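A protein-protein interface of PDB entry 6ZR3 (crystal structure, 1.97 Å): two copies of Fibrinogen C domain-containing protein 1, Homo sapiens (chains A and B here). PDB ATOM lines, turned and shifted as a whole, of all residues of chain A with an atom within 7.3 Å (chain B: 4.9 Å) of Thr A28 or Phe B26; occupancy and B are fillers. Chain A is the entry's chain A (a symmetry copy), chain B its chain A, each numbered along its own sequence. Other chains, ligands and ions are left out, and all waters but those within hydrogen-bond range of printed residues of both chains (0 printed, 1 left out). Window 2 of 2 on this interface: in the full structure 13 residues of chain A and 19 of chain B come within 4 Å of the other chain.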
ATOM      1  N   ARG A   5     -27.260  -6.462  31.522  1.00  0.00           N
ATOM      2  CA  ARG A   5     -26.407  -6.976  30.413  1.00  0.00           C
ATOM      3  C   ARG A   5     -27.287  -7.479  29.271  1.00  0.00           C
ATOM      4  O   ARG A   5     -27.397  -8.678  29.035  1.00  0.00           O
ATOM      5  CB  ARG A   5     -25.449  -8.054  30.922  1.00  0.00           C
ATOM      6  CG  ARG A   5     -24.368  -7.507  31.840  1.00  0.00           C
ATOM      7  CD  ARG A   5     -23.544  -8.640  32.418  1.00  0.00           C
ATOM      8  NE  ARG A   5     -22.705  -9.271  31.406  1.00  0.00           N
ATOM      9  CZ  ARG A   5     -21.591  -8.742  30.895  1.00  0.00           C
ATOM     10  NH1 ARG A   5     -21.175  -7.544  31.284  1.00  0.00           N
ATOM     11  NH2 ARG A   5     -20.906  -9.408  29.979  1.00  0.00           N
ATOM     12  N   ARG A   7     -28.120  -8.582  25.595  1.00  0.00           N
ATOM     13  CA  ARG A   7     -27.267  -9.314  24.622  1.00  0.00           C
ATOM     14  C   ARG A   7     -27.373  -8.650  23.242  1.00  0.00           C
ATOM     15  O   ARG A   7     -26.554  -8.983  22.367  1.00  0.00           O
ATOM     16  CB  ARG A   7     -27.663 -10.791  24.563  1.00  0.00           C
ATOM     17  CG  ARG A   7     -28.842 -11.076  23.645  1.00  0.00           C
ATOM     18  CD  ARG A   7     -29.282 -12.531  23.626  1.00  0.00           C
ATOM     19  NE  ARG A   7     -30.551 -12.678  22.917  1.00  0.00           N
ATOM     20  CZ  ARG A   7     -31.252 -13.808  22.842  1.00  0.00           C
ATOM     21  NH1 ARG A   7     -30.800 -14.910  23.423  1.00  0.00           N
ATOM     22  NH2 ARG A   7     -32.398 -13.833  22.181  1.00  0.00           N
ATOM     23  N   PHE A  26     -23.920  -6.944  25.116  1.00  0.00           N
ATOM     24  CA  PHE A  26     -22.926  -7.903  25.665  1.00  0.00           C
ATOM     25  C   PHE A  26     -23.236  -9.298  25.150  1.00  0.00           C
ATOM     26  O   PHE A  26     -23.925 -10.073  25.808  1.00  0.00           O
ATOM     27  CB  PHE A  26     -22.955  -7.869  27.193  1.00  0.00           C
ATOM     28  CG  PHE A  26     -22.808  -6.489  27.769  1.00  0.00           C
ATOM     29  CD1 PHE A  26     -23.917  -5.667  27.924  1.00  0.00           C
ATOM     30  CD2 PHE A  26     -21.570  -6.014  28.161  1.00  0.00           C
ATOM     31  CE1 PHE A  26     -23.788  -4.396  28.462  1.00  0.00           C
ATOM     32  CE2 PHE A  26     -21.442  -4.737  28.687  1.00  0.00           C
ATOM     33  CZ  PHE A  26     -22.551  -3.934  28.841  1.00  0.00           C
ATOM     34  N   PRO A  27     -22.809  -9.633  23.918  1.00  0.00           N
ATOM     35  CA  PRO A  27     -23.058 -10.966  23.372  1.00  0.00           C
ATOM     36  C   PRO A  27     -22.398 -12.054  24.233  1.00  0.00           C
ATOM     37  O   PRO A  27     -21.435 -11.782  24.948  1.00  0.00           O
ATOM     38  CB  PRO A  27     -22.486 -10.885  21.948  1.00  0.00           C
ATOM     39  CG  PRO A  27     -22.481  -9.399  21.639  1.00  0.00           C
ATOM     40  CD  PRO A  27     -22.160  -8.734  22.957  1.00  0.00           C
ATOM     41  N   THR A  28     -22.963 -13.262  24.161  1.00  0.00           N
ATOM     42  CA  THR A  28     -22.567 -14.452  24.957  1.00  0.00           C
ATOM     43  C   THR A  28     -21.042 -14.652  24.916  1.00  0.00           C
ATOM     44  O   THR A  28     -20.452 -14.862  25.988  1.00  0.00           O
ATOM     45  CB  THR A  28     -23.312 -15.695  24.455  1.00  0.00           C
ATOM     46  OG1 THR A  28     -24.713 -15.459  24.622  1.00  0.00           O
ATOM     47  CG2 THR A  28     -22.936 -16.957  25.198  1.00  0.00           C
ATOM     48  N   HIS A  29     -20.424 -14.640  23.733  1.00  0.00           N
ATOM     49  CA  HIS A  29     -18.971 -14.913  23.568  1.00  0.00           C
ATOM     50  C   HIS A  29     -18.183 -13.625  23.322  1.00  0.00           C
ATOM     51  O   HIS A  29     -17.019 -13.746  22.897  1.00  0.00           O
ATOM     52  CB  HIS A  29     -18.728 -15.963  22.475  1.00  0.00           C
ATOM     53  CG  HIS A  29     -19.372 -17.269  22.800  1.00  0.00           C
ATOM     54  ND1 HIS A  29     -19.150 -17.912  23.999  1.00  0.00           N
ATOM     55  CD2 HIS A  29     -20.258 -18.026  22.117  1.00  0.00           C
ATOM     56  CE1 HIS A  29     -19.858 -19.028  24.030  1.00  0.00           C
ATOM     57  NE2 HIS A  29     -20.554 -19.120  22.886  1.00  0.00           N
ATOM     58  N   TYR A  30     -18.754 -12.453  23.631  1.00  0.00           N
ATOM     59  CA  TYR A  30     -18.065 -11.134  23.553  1.00  0.00           C
ATOM     60  C   TYR A  30     -18.397 -10.367  24.833  1.00  0.00           C
ATOM     61  O   TYR A  30     -19.020  -9.309  24.802  1.00  0.00           O
ATOM     62  CB  TYR A  30     -18.467 -10.435  22.251  1.00  0.00           C
ATOM     63  CG  TYR A  30     -17.490  -9.431  21.689  1.00  0.00           C
ATOM     64  CD1 TYR A  30     -17.022  -8.360  22.441  1.00  0.00           C
ATOM     65  CD2 TYR A  30     -17.077  -9.521  20.366  1.00  0.00           C
ATOM     66  CE1 TYR A  30     -16.130  -7.438  21.910  1.00  0.00           C
ATOM     67  CE2 TYR A  30     -16.202  -8.599  19.814  1.00  0.00           C
ATOM     68  CZ  TYR A  30     -15.725  -7.554  20.588  1.00  0.00           C
ATOM     69  OH  TYR A  30     -14.875  -6.640  20.027  1.00  0.00           O
ATOM     70  N   PRO A  31     -17.998 -10.893  26.012  1.00  0.00           N
ATOM     71  CA  PRO A  31     -18.526 -10.399  27.284  1.00  0.00           C
ATOM     72  C   PRO A  31     -18.045  -8.988  27.680  1.00  0.00           C
ATOM     73  O   PRO A  31     -18.736  -8.367  28.457  1.00  0.00           O
ATOM     74  CB  PRO A  31     -18.075 -11.473  28.290  1.00  0.00           C
ATOM     75  CG  PRO A  31     -16.821 -12.064  27.684  1.00  0.00           C
ATOM     76  CD  PRO A  31     -17.006 -11.963  26.183  1.00  0.00           C
ATOM     77  N   ALA A  87     -20.410 -12.386  16.658  1.00  0.00           N
ATOM     78  CA  ALA A  87     -20.717 -12.513  18.104  1.00  0.00           C
ATOM     79  C   ALA A  87     -22.233 -12.402  18.319  1.00  0.00           C
ATOM     80  O   ALA A  87     -22.774 -13.139  19.152  1.00  0.00           O
ATOM     81  CB  ALA A  87     -19.956 -11.485  18.896  1.00  0.00           C
ATOM     82  N   LEU A  88     -22.901 -11.526  17.574  1.00  0.00           N
ATOM     83  CA  LEU A  88     -24.366 -11.326  17.675  1.00  0.00           C
ATOM     84  C   LEU A  88     -25.108 -12.521  17.064  1.00  0.00           C
ATOM     85  O   LEU A  88     -25.918 -13.115  17.779  1.00  0.00           O
ATOM     86  CB  LEU A  88     -24.743 -10.013  16.994  1.00  0.00           C
ATOM     87  CG  LEU A  88     -24.338  -8.767  17.766  1.00  0.00           C
ATOM     88  CD1 LEU A  88     -24.391  -7.542  16.875  1.00  0.00           C
ATOM     89  CD2 LEU A  88     -25.191  -8.578  19.010  1.00  0.00           C
ATOM     90  N   THR A  90     -24.420 -15.624  16.210  1.00  0.00           N
ATOM     91  CA  THR A  90     -24.176 -17.007  16.707  1.00  0.00           C
ATOM     92  C   THR A  90     -24.816 -17.240  18.084  1.00  0.00           C
ATOM     93  O   THR A  90     -24.843 -18.407  18.488  1.00  0.00           O
ATOM     94  CB  THR A  90     -22.684 -17.345  16.821  1.00  0.00           C
ATOM     95  OG1 THR A  90     -22.074 -16.339  17.621  1.00  0.00           O
ATOM     96  CG2 THR A  90     -21.982 -17.424  15.489  1.00  0.00           C
ATOM     97  N   GLN A  91     -25.268 -16.201  18.797  1.00  0.00           N
ATOM     98  CA  GLN A  91     -25.764 -16.328  20.197  1.00  0.00           C
ATOM     99  C   GLN A  91     -27.251 -16.708  20.211  1.00  0.00           C
ATOM    100  O   GLN A  91     -27.741 -17.142  21.283  1.00  0.00           O
ATOM    101  CB  GLN A  91     -25.508 -15.056  21.013  1.00  0.00           C
ATOM    102  CG  GLN A  91     -26.419 -13.874  20.710  1.00  0.00           C
ATOM    103  CD  GLN A  91     -26.076 -12.664  21.552  1.00  0.00           C
ATOM    104  OE1 GLN A  91     -25.528 -12.775  22.654  1.00  0.00           O
ATOM    105  NE2 GLN A  91     -26.415 -11.487  21.052  1.00  0.00           N
ATOM    106  N   ALA A  92     -27.936 -16.534  19.078  1.00  0.00           N
ATOM    107  CA  ALA A  92     -29.379 -16.808  18.878  1.00  0.00           C
ATOM    108  C   ALA A  92     -29.675 -16.777  17.374  1.00  0.00           C
ATOM    109  O   ALA A  92     -28.754 -16.460  16.598  1.00  0.00           O
ATOM    110  CB  ALA A  92     -30.213 -15.811  19.644  1.00  0.00           C
ATOM    111  N   SER B   4     -26.381 -22.324  33.069  1.00  0.00           N
ATOM    112  CA  SER B   4     -26.135 -20.956  32.513  1.00  0.00           C
ATOM    113  C   SER B   4     -24.731 -20.873  31.893  1.00  0.00           C
ATOM    114  O   SER B   4     -24.624 -20.341  30.765  1.00  0.00           O
ATOM    115  CB  SER B   4     -26.336 -19.896  33.571  1.00  0.00           C
ATOM    116  OG  SER B   4     -26.293 -18.598  32.995  1.00  0.00           O
ATOM    117  N   ARG B   5     -23.703 -21.358  32.607  1.00  0.00           N
ATOM    118  CA  ARG B   5     -22.289 -21.380  32.136  1.00  0.00           C
ATOM    119  C   ARG B   5     -21.711 -22.784  32.293  1.00  0.00           C
ATOM    120  O   ARG B   5     -20.872 -23.032  33.154  1.00  0.00           O
ATOM    121  CB  ARG B   5     -21.457 -20.326  32.869  1.00  0.00           C
ATOM    122  CG  ARG B   5     -21.829 -18.902  32.490  1.00  0.00           C
ATOM    123  CD  ARG B   5     -21.071 -17.913  33.351  1.00  0.00           C
ATOM    124  NE  ARG B   5     -19.649 -17.887  33.024  1.00  0.00           N
ATOM    125  CZ  ARG B   5     -19.124 -17.320  31.936  1.00  0.00           C
ATOM    126  NH1 ARG B   5     -19.904 -16.736  31.037  1.00  0.00           N
ATOM    127  NH2 ARG B   5     -17.815 -17.357  31.743  1.00  0.00           N
ATOM    128  N   PRO B   6     -22.136 -23.740  31.441  1.00  0.00           N
ATOM    129  CA  PRO B   6     -21.541 -25.073  31.426  1.00  0.00           C
ATOM    130  C   PRO B   6     -20.067 -24.947  31.015  1.00  0.00           C
ATOM    131  O   PRO B   6     -19.775 -24.133  30.162  1.00  0.00           O
ATOM    132  CB  PRO B   6     -22.390 -25.842  30.407  1.00  0.00           C
ATOM    133  CG  PRO B   6     -22.974 -24.766  29.508  1.00  0.00           C
ATOM    134  CD  PRO B   6     -23.178 -23.575  30.416  1.00  0.00           C
ATOM    135  N   ARG B   7     -19.191 -25.725  31.642  1.00  0.00           N
ATOM    136  CA  ARG B   7     -17.724 -25.666  31.408  1.00  0.00           C
ATOM    137  C   ARG B   7     -17.351 -26.594  30.244  1.00  0.00           C
ATOM    138  O   ARG B   7     -16.209 -26.496  29.759  1.00  0.00           O
ATOM    139  CB  ARG B   7     -16.960 -26.034  32.682  1.00  0.00           C
ATOM    140  CG  ARG B   7     -16.801 -27.532  32.893  1.00  0.00           C
ATOM    141  CD  ARG B   7     -16.097 -27.909  34.187  1.00  0.00           C
ATOM    142  NE  ARG B   7     -16.194 -29.346  34.429  1.00  0.00           N
ATOM    143  CZ  ARG B   7     -15.786 -29.959  35.539  1.00  0.00           C
ATOM    144  NH1 ARG B   7     -15.231 -29.260  36.518  1.00  0.00           N
ATOM    145  NH2 ARG B   7     -15.929 -31.268  35.663  1.00  0.00           N
ATOM    146  N   SER B  24     -22.661 -23.648  23.463  1.00  0.00           N
ATOM    147  CA  SER B  24     -21.732 -22.727  24.155  1.00  0.00           C
ATOM    148  C   SER B  24     -21.198 -23.408  25.411  1.00  0.00           C
ATOM    149  O   SER B  24     -22.018 -23.921  26.192  1.00  0.00           O
ATOM    150  CB  SER B  24     -22.426 -21.454  24.501  1.00  0.00           C
ATOM    151  OG  SER B  24     -22.638 -20.692  23.330  1.00  0.00           O
ATOM    152  N   VAL B  25     -19.875 -23.394  25.584  1.00  0.00           N
ATOM    153  CA  VAL B  25     -19.184 -23.833  26.826  1.00  0.00           C
ATOM    154  C   VAL B  25     -18.214 -22.725  27.254  1.00  0.00           C
ATOM    155  O   VAL B  25     -17.826 -21.897  26.401  1.00  0.00           O
ATOM    156  CB  VAL B  25     -18.494 -25.194  26.637  1.00  0.00           C
ATOM    157  CG1 VAL B  25     -19.510 -26.268  26.276  1.00  0.00           C
ATOM    158  CG2 VAL B  25     -17.363 -25.149  25.622  1.00  0.00           C
ATOM    159  N   PHE B  26     -17.867 -22.699  28.538  1.00  0.00           N
ATOM    160  CA  PHE B  26     -17.115 -21.591  29.185  1.00  0.00           C
ATOM    161  C   PHE B  26     -16.083 -22.171  30.136  1.00  0.00           C
ATOM    162  O   PHE B  26     -16.337 -22.316  31.329  1.00  0.00           O
ATOM    163  CB  PHE B  26     -18.081 -20.669  29.929  1.00  0.00           C
ATOM    164  CG  PHE B  26     -19.221 -20.179  29.081  1.00  0.00           C
ATOM    165  CD1 PHE B  26     -20.371 -20.943  28.935  1.00  0.00           C
ATOM    166  CD2 PHE B  26     -19.150 -18.957  28.438  1.00  0.00           C
ATOM    167  CE1 PHE B  26     -21.429 -20.492  28.161  1.00  0.00           C
ATOM    168  CE2 PHE B  26     -20.205 -18.514  27.654  1.00  0.00           C
ATOM    169  CZ  PHE B  26     -21.343 -19.280  27.522  1.00  0.00           C
ATOM    170  N   PRO B  27     -14.914 -22.602  29.624  1.00  0.00           N
ATOM    171  CA  PRO B  27     -13.872 -23.153  30.487  1.00  0.00           C
ATOM    172  C   PRO B  27     -13.394 -22.116  31.517  1.00  0.00           C
ATOM    173  O   PRO B  27     -13.528 -20.913  31.296  1.00  0.00           O
ATOM    174  CB  PRO B  27     -12.775 -23.582  29.500  1.00  0.00           C
ATOM    175  CG  PRO B  27     -13.512 -23.749  28.184  1.00  0.00           C
ATOM    176  CD  PRO B  27     -14.573 -22.673  28.199  1.00  0.00           C
ATOM    177  N   THR B  28     -12.873 -22.621  32.638  1.00  0.00           N
ATOM    178  CA  THR B  28     -12.421 -21.834  33.813  1.00  0.00           C
ATOM    179  C   THR B  28     -11.525 -20.663  33.374  1.00  0.00           C
ATOM    180  O   THR B  28     -11.758 -19.540  33.848  1.00  0.00           O
ATOM    181  CB  THR B  28     -11.704 -22.746  34.817  1.00  0.00           C
ATOM    182  OG1 THR B  28     -12.639 -23.741  35.244  1.00  0.00           O
ATOM    183  CG2 THR B  28     -11.185 -22.008  36.029  1.00  0.00           C
ATOM    184  N   TYR B  30     -10.995 -19.630  30.153  1.00  0.00           N
ATOM    185  CA  TYR B  30     -11.433 -19.119  28.824  1.00  0.00           C
ATOM    186  C   TYR B  30     -12.854 -18.578  28.986  1.00  0.00           C
ATOM    187  O   TYR B  30     -13.800 -19.073  28.379  1.00  0.00           O
ATOM    188  CB  TYR B  30     -11.273 -20.230  27.782  1.00  0.00           C
ATOM    189  CG  TYR B  30     -11.079 -19.796  26.350  1.00  0.00           C
ATOM    190  CD1 TYR B  30     -11.976 -18.949  25.710  1.00  0.00           C
ATOM    191  CD2 TYR B  30     -10.015 -20.291  25.606  1.00  0.00           C
ATOM    192  CE1 TYR B  30     -11.792 -18.564  24.389  1.00  0.00           C
ATOM    193  CE2 TYR B  30      -9.827 -19.932  24.281  1.00  0.00           C
ATOM    194  CZ  TYR B  30     -10.717 -19.065  23.669  1.00  0.00           C
ATOM    195  OH  TYR B  30     -10.529 -18.730  22.356  1.00  0.00           O
ATOM    196  N   PRO B  31     -13.048 -17.543  29.833  1.00  0.00           N
ATOM    197  CA  PRO B  31     -14.390 -17.165  30.278  1.00  0.00           C
ATOM    198  C   PRO B  31     -15.276 -16.523  29.191  1.00  0.00           C
ATOM    199  O   PRO B  31     -16.475 -16.578  29.354  1.00  0.00           O
ATOM    200  CB  PRO B  31     -14.111 -16.204  31.447  1.00  0.00           C
ATOM    201  CG  PRO B  31     -12.760 -15.600  31.134  1.00  0.00           C
ATOM    202  CD  PRO B  31     -11.999 -16.672  30.379  1.00  0.00           C
ATOM    203  N   ALA B  32     -14.700 -16.009  28.098  1.00  0.00           N
ATOM    204  CA  ALA B  32     -15.444 -15.581  26.888  1.00  0.00           C
ATOM    205  C   ALA B  32     -16.272 -16.766  26.371  1.00  0.00           C
ATOM    206  O   ALA B  32     -17.394 -16.554  25.863  1.00  0.00           O
ATOM    207  CB  ALA B  32     -14.496 -15.075  25.824  1.00  0.00           C
ATOM    208  N   GLY B  33     -15.720 -17.970  26.511  1.00  0.00           N
ATOM    209  CA  GLY B  33     -16.336 -19.217  26.037  1.00  0.00           C
ATOM    210  C   GLY B  33     -16.240 -19.339  24.527  1.00  0.00           C
ATOM    211  O   GLY B  33     -15.745 -18.405  23.857  1.00  0.00           O
ATOM    212  N   GLN B  91      -8.900 -27.788  33.137  1.00  0.00           N
ATOM    213  CA  GLN B  91      -9.917 -27.313  34.120  1.00  0.00           C
ATOM    214  C   GLN B  91     -10.415 -28.479  34.985  1.00  0.00           C
ATOM    215  O   GLN B  91     -11.037 -28.207  36.043  1.00  0.00           O
ATOM    216  CB  GLN B  91     -11.082 -26.591  33.435  1.00  0.00           C
ATOM    217  CG  GLN B  91     -12.081 -27.478  32.706  1.00  0.00           C
ATOM    218  CD  GLN B  91     -13.181 -26.673  32.049  1.00  0.00           C
ATOM    219  OE1 GLN B  91     -13.514 -25.562  32.477  1.00  0.00           O
ATOM    220  NE2 GLN B  91     -13.777 -27.233  31.009  1.00  0.00           N
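Thr A28 touches Phe B26, but with the chains exchanged Phe A26 does not touch Thr B28 (17.4 Å). Positions printed for both chains: 5, 7, 26, 27, 28, 30, 31 and 91.
Hydrophobic or aromatic side chains of chain A within 4 Å of the printed part of chain B: His A29 and Pro A31. Of the 14 printed residues of chain B, 4 touch a printed residue of chain A. Hydrophobic or aromatic side chains of chain B within 4 Å of the printed part of chain A: Phe B26. Among the printed residues, 7 pairs touch across the chains. Among the printed residues, no Asp or Glu carboxylate lies within 4 Å of a Lys or Arg side-chain nitrogen of the other chain.
CZ of Phe B26 touches CG2 of Thr A28, 3.7 Å away. CE1 of His A29 touches CE2 of Phe B26 (3.7 Å). Pro A31 touches Ala B32 (CG to CA, 3.9 Å).
The backbone NH of Thr A28 sits at hydrogen-bond distance from the side-chain amide oxygen of Gln A91 (3.0 Å). The backbone carbonyl oxygen of Pro B6 sits at hydrogen-bond distance from the backbone NH of Phe B26 (2.9 Å). The guanidinium group (NH2) of Arg A5 lies within hydrogen-bond range of the backbone carbonyl oxygen (O) of Pro A31 (2.8 Å).
OG of Ser B24 is in hydrogen-bond range of NE2 of His A29, 2.6 Å away. The backbone carbonyl oxygen (O) of Ala B32 is in hydrogen-bond range of a ring nitrogen (ND1) of His A29 (2.9 Å). O of Thr A28 lies close to O of Ala B32 (3.5 Å). A ring nitrogen (ND1) of His A29 sits close to the backbone carbonyl oxygen (O) of Gly B33.
Thr A28 touches just these residues of chain B: Phe B26 and Ala B32. Of the printed residues of chain A, Gly B33 touches His A29 (3.3 Å). Printed residues of chain A within 4 Å of Ser B24: His A29. Of the printed residues of chain A, Ala B32 touches Thr A28 (3.5 Å), His A29 (2.9 Å) and Pro A31 (3.9 Å). Of the printed residues of chain B, Pro A31 touches Ala B32. Of the printed residues of chain B, His A29 touches Ser B24 (2.6 Å), Phe B26 (3.7 Å), Ala B32 (2.9 Å) and Gly B33 (3.3 Å). Arg A5 touches none of the printed residues of chain B. The nearest residue of chain B that does not touch Thr A28 is Ser B24 (4.2 Å). The nearest printed residue of chain A that does not touch Phe B26 is Pro A31 (7.3 Å). The nearest printed residue of chain B that does not touch His A29 is Val B25 (4.2 Å).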
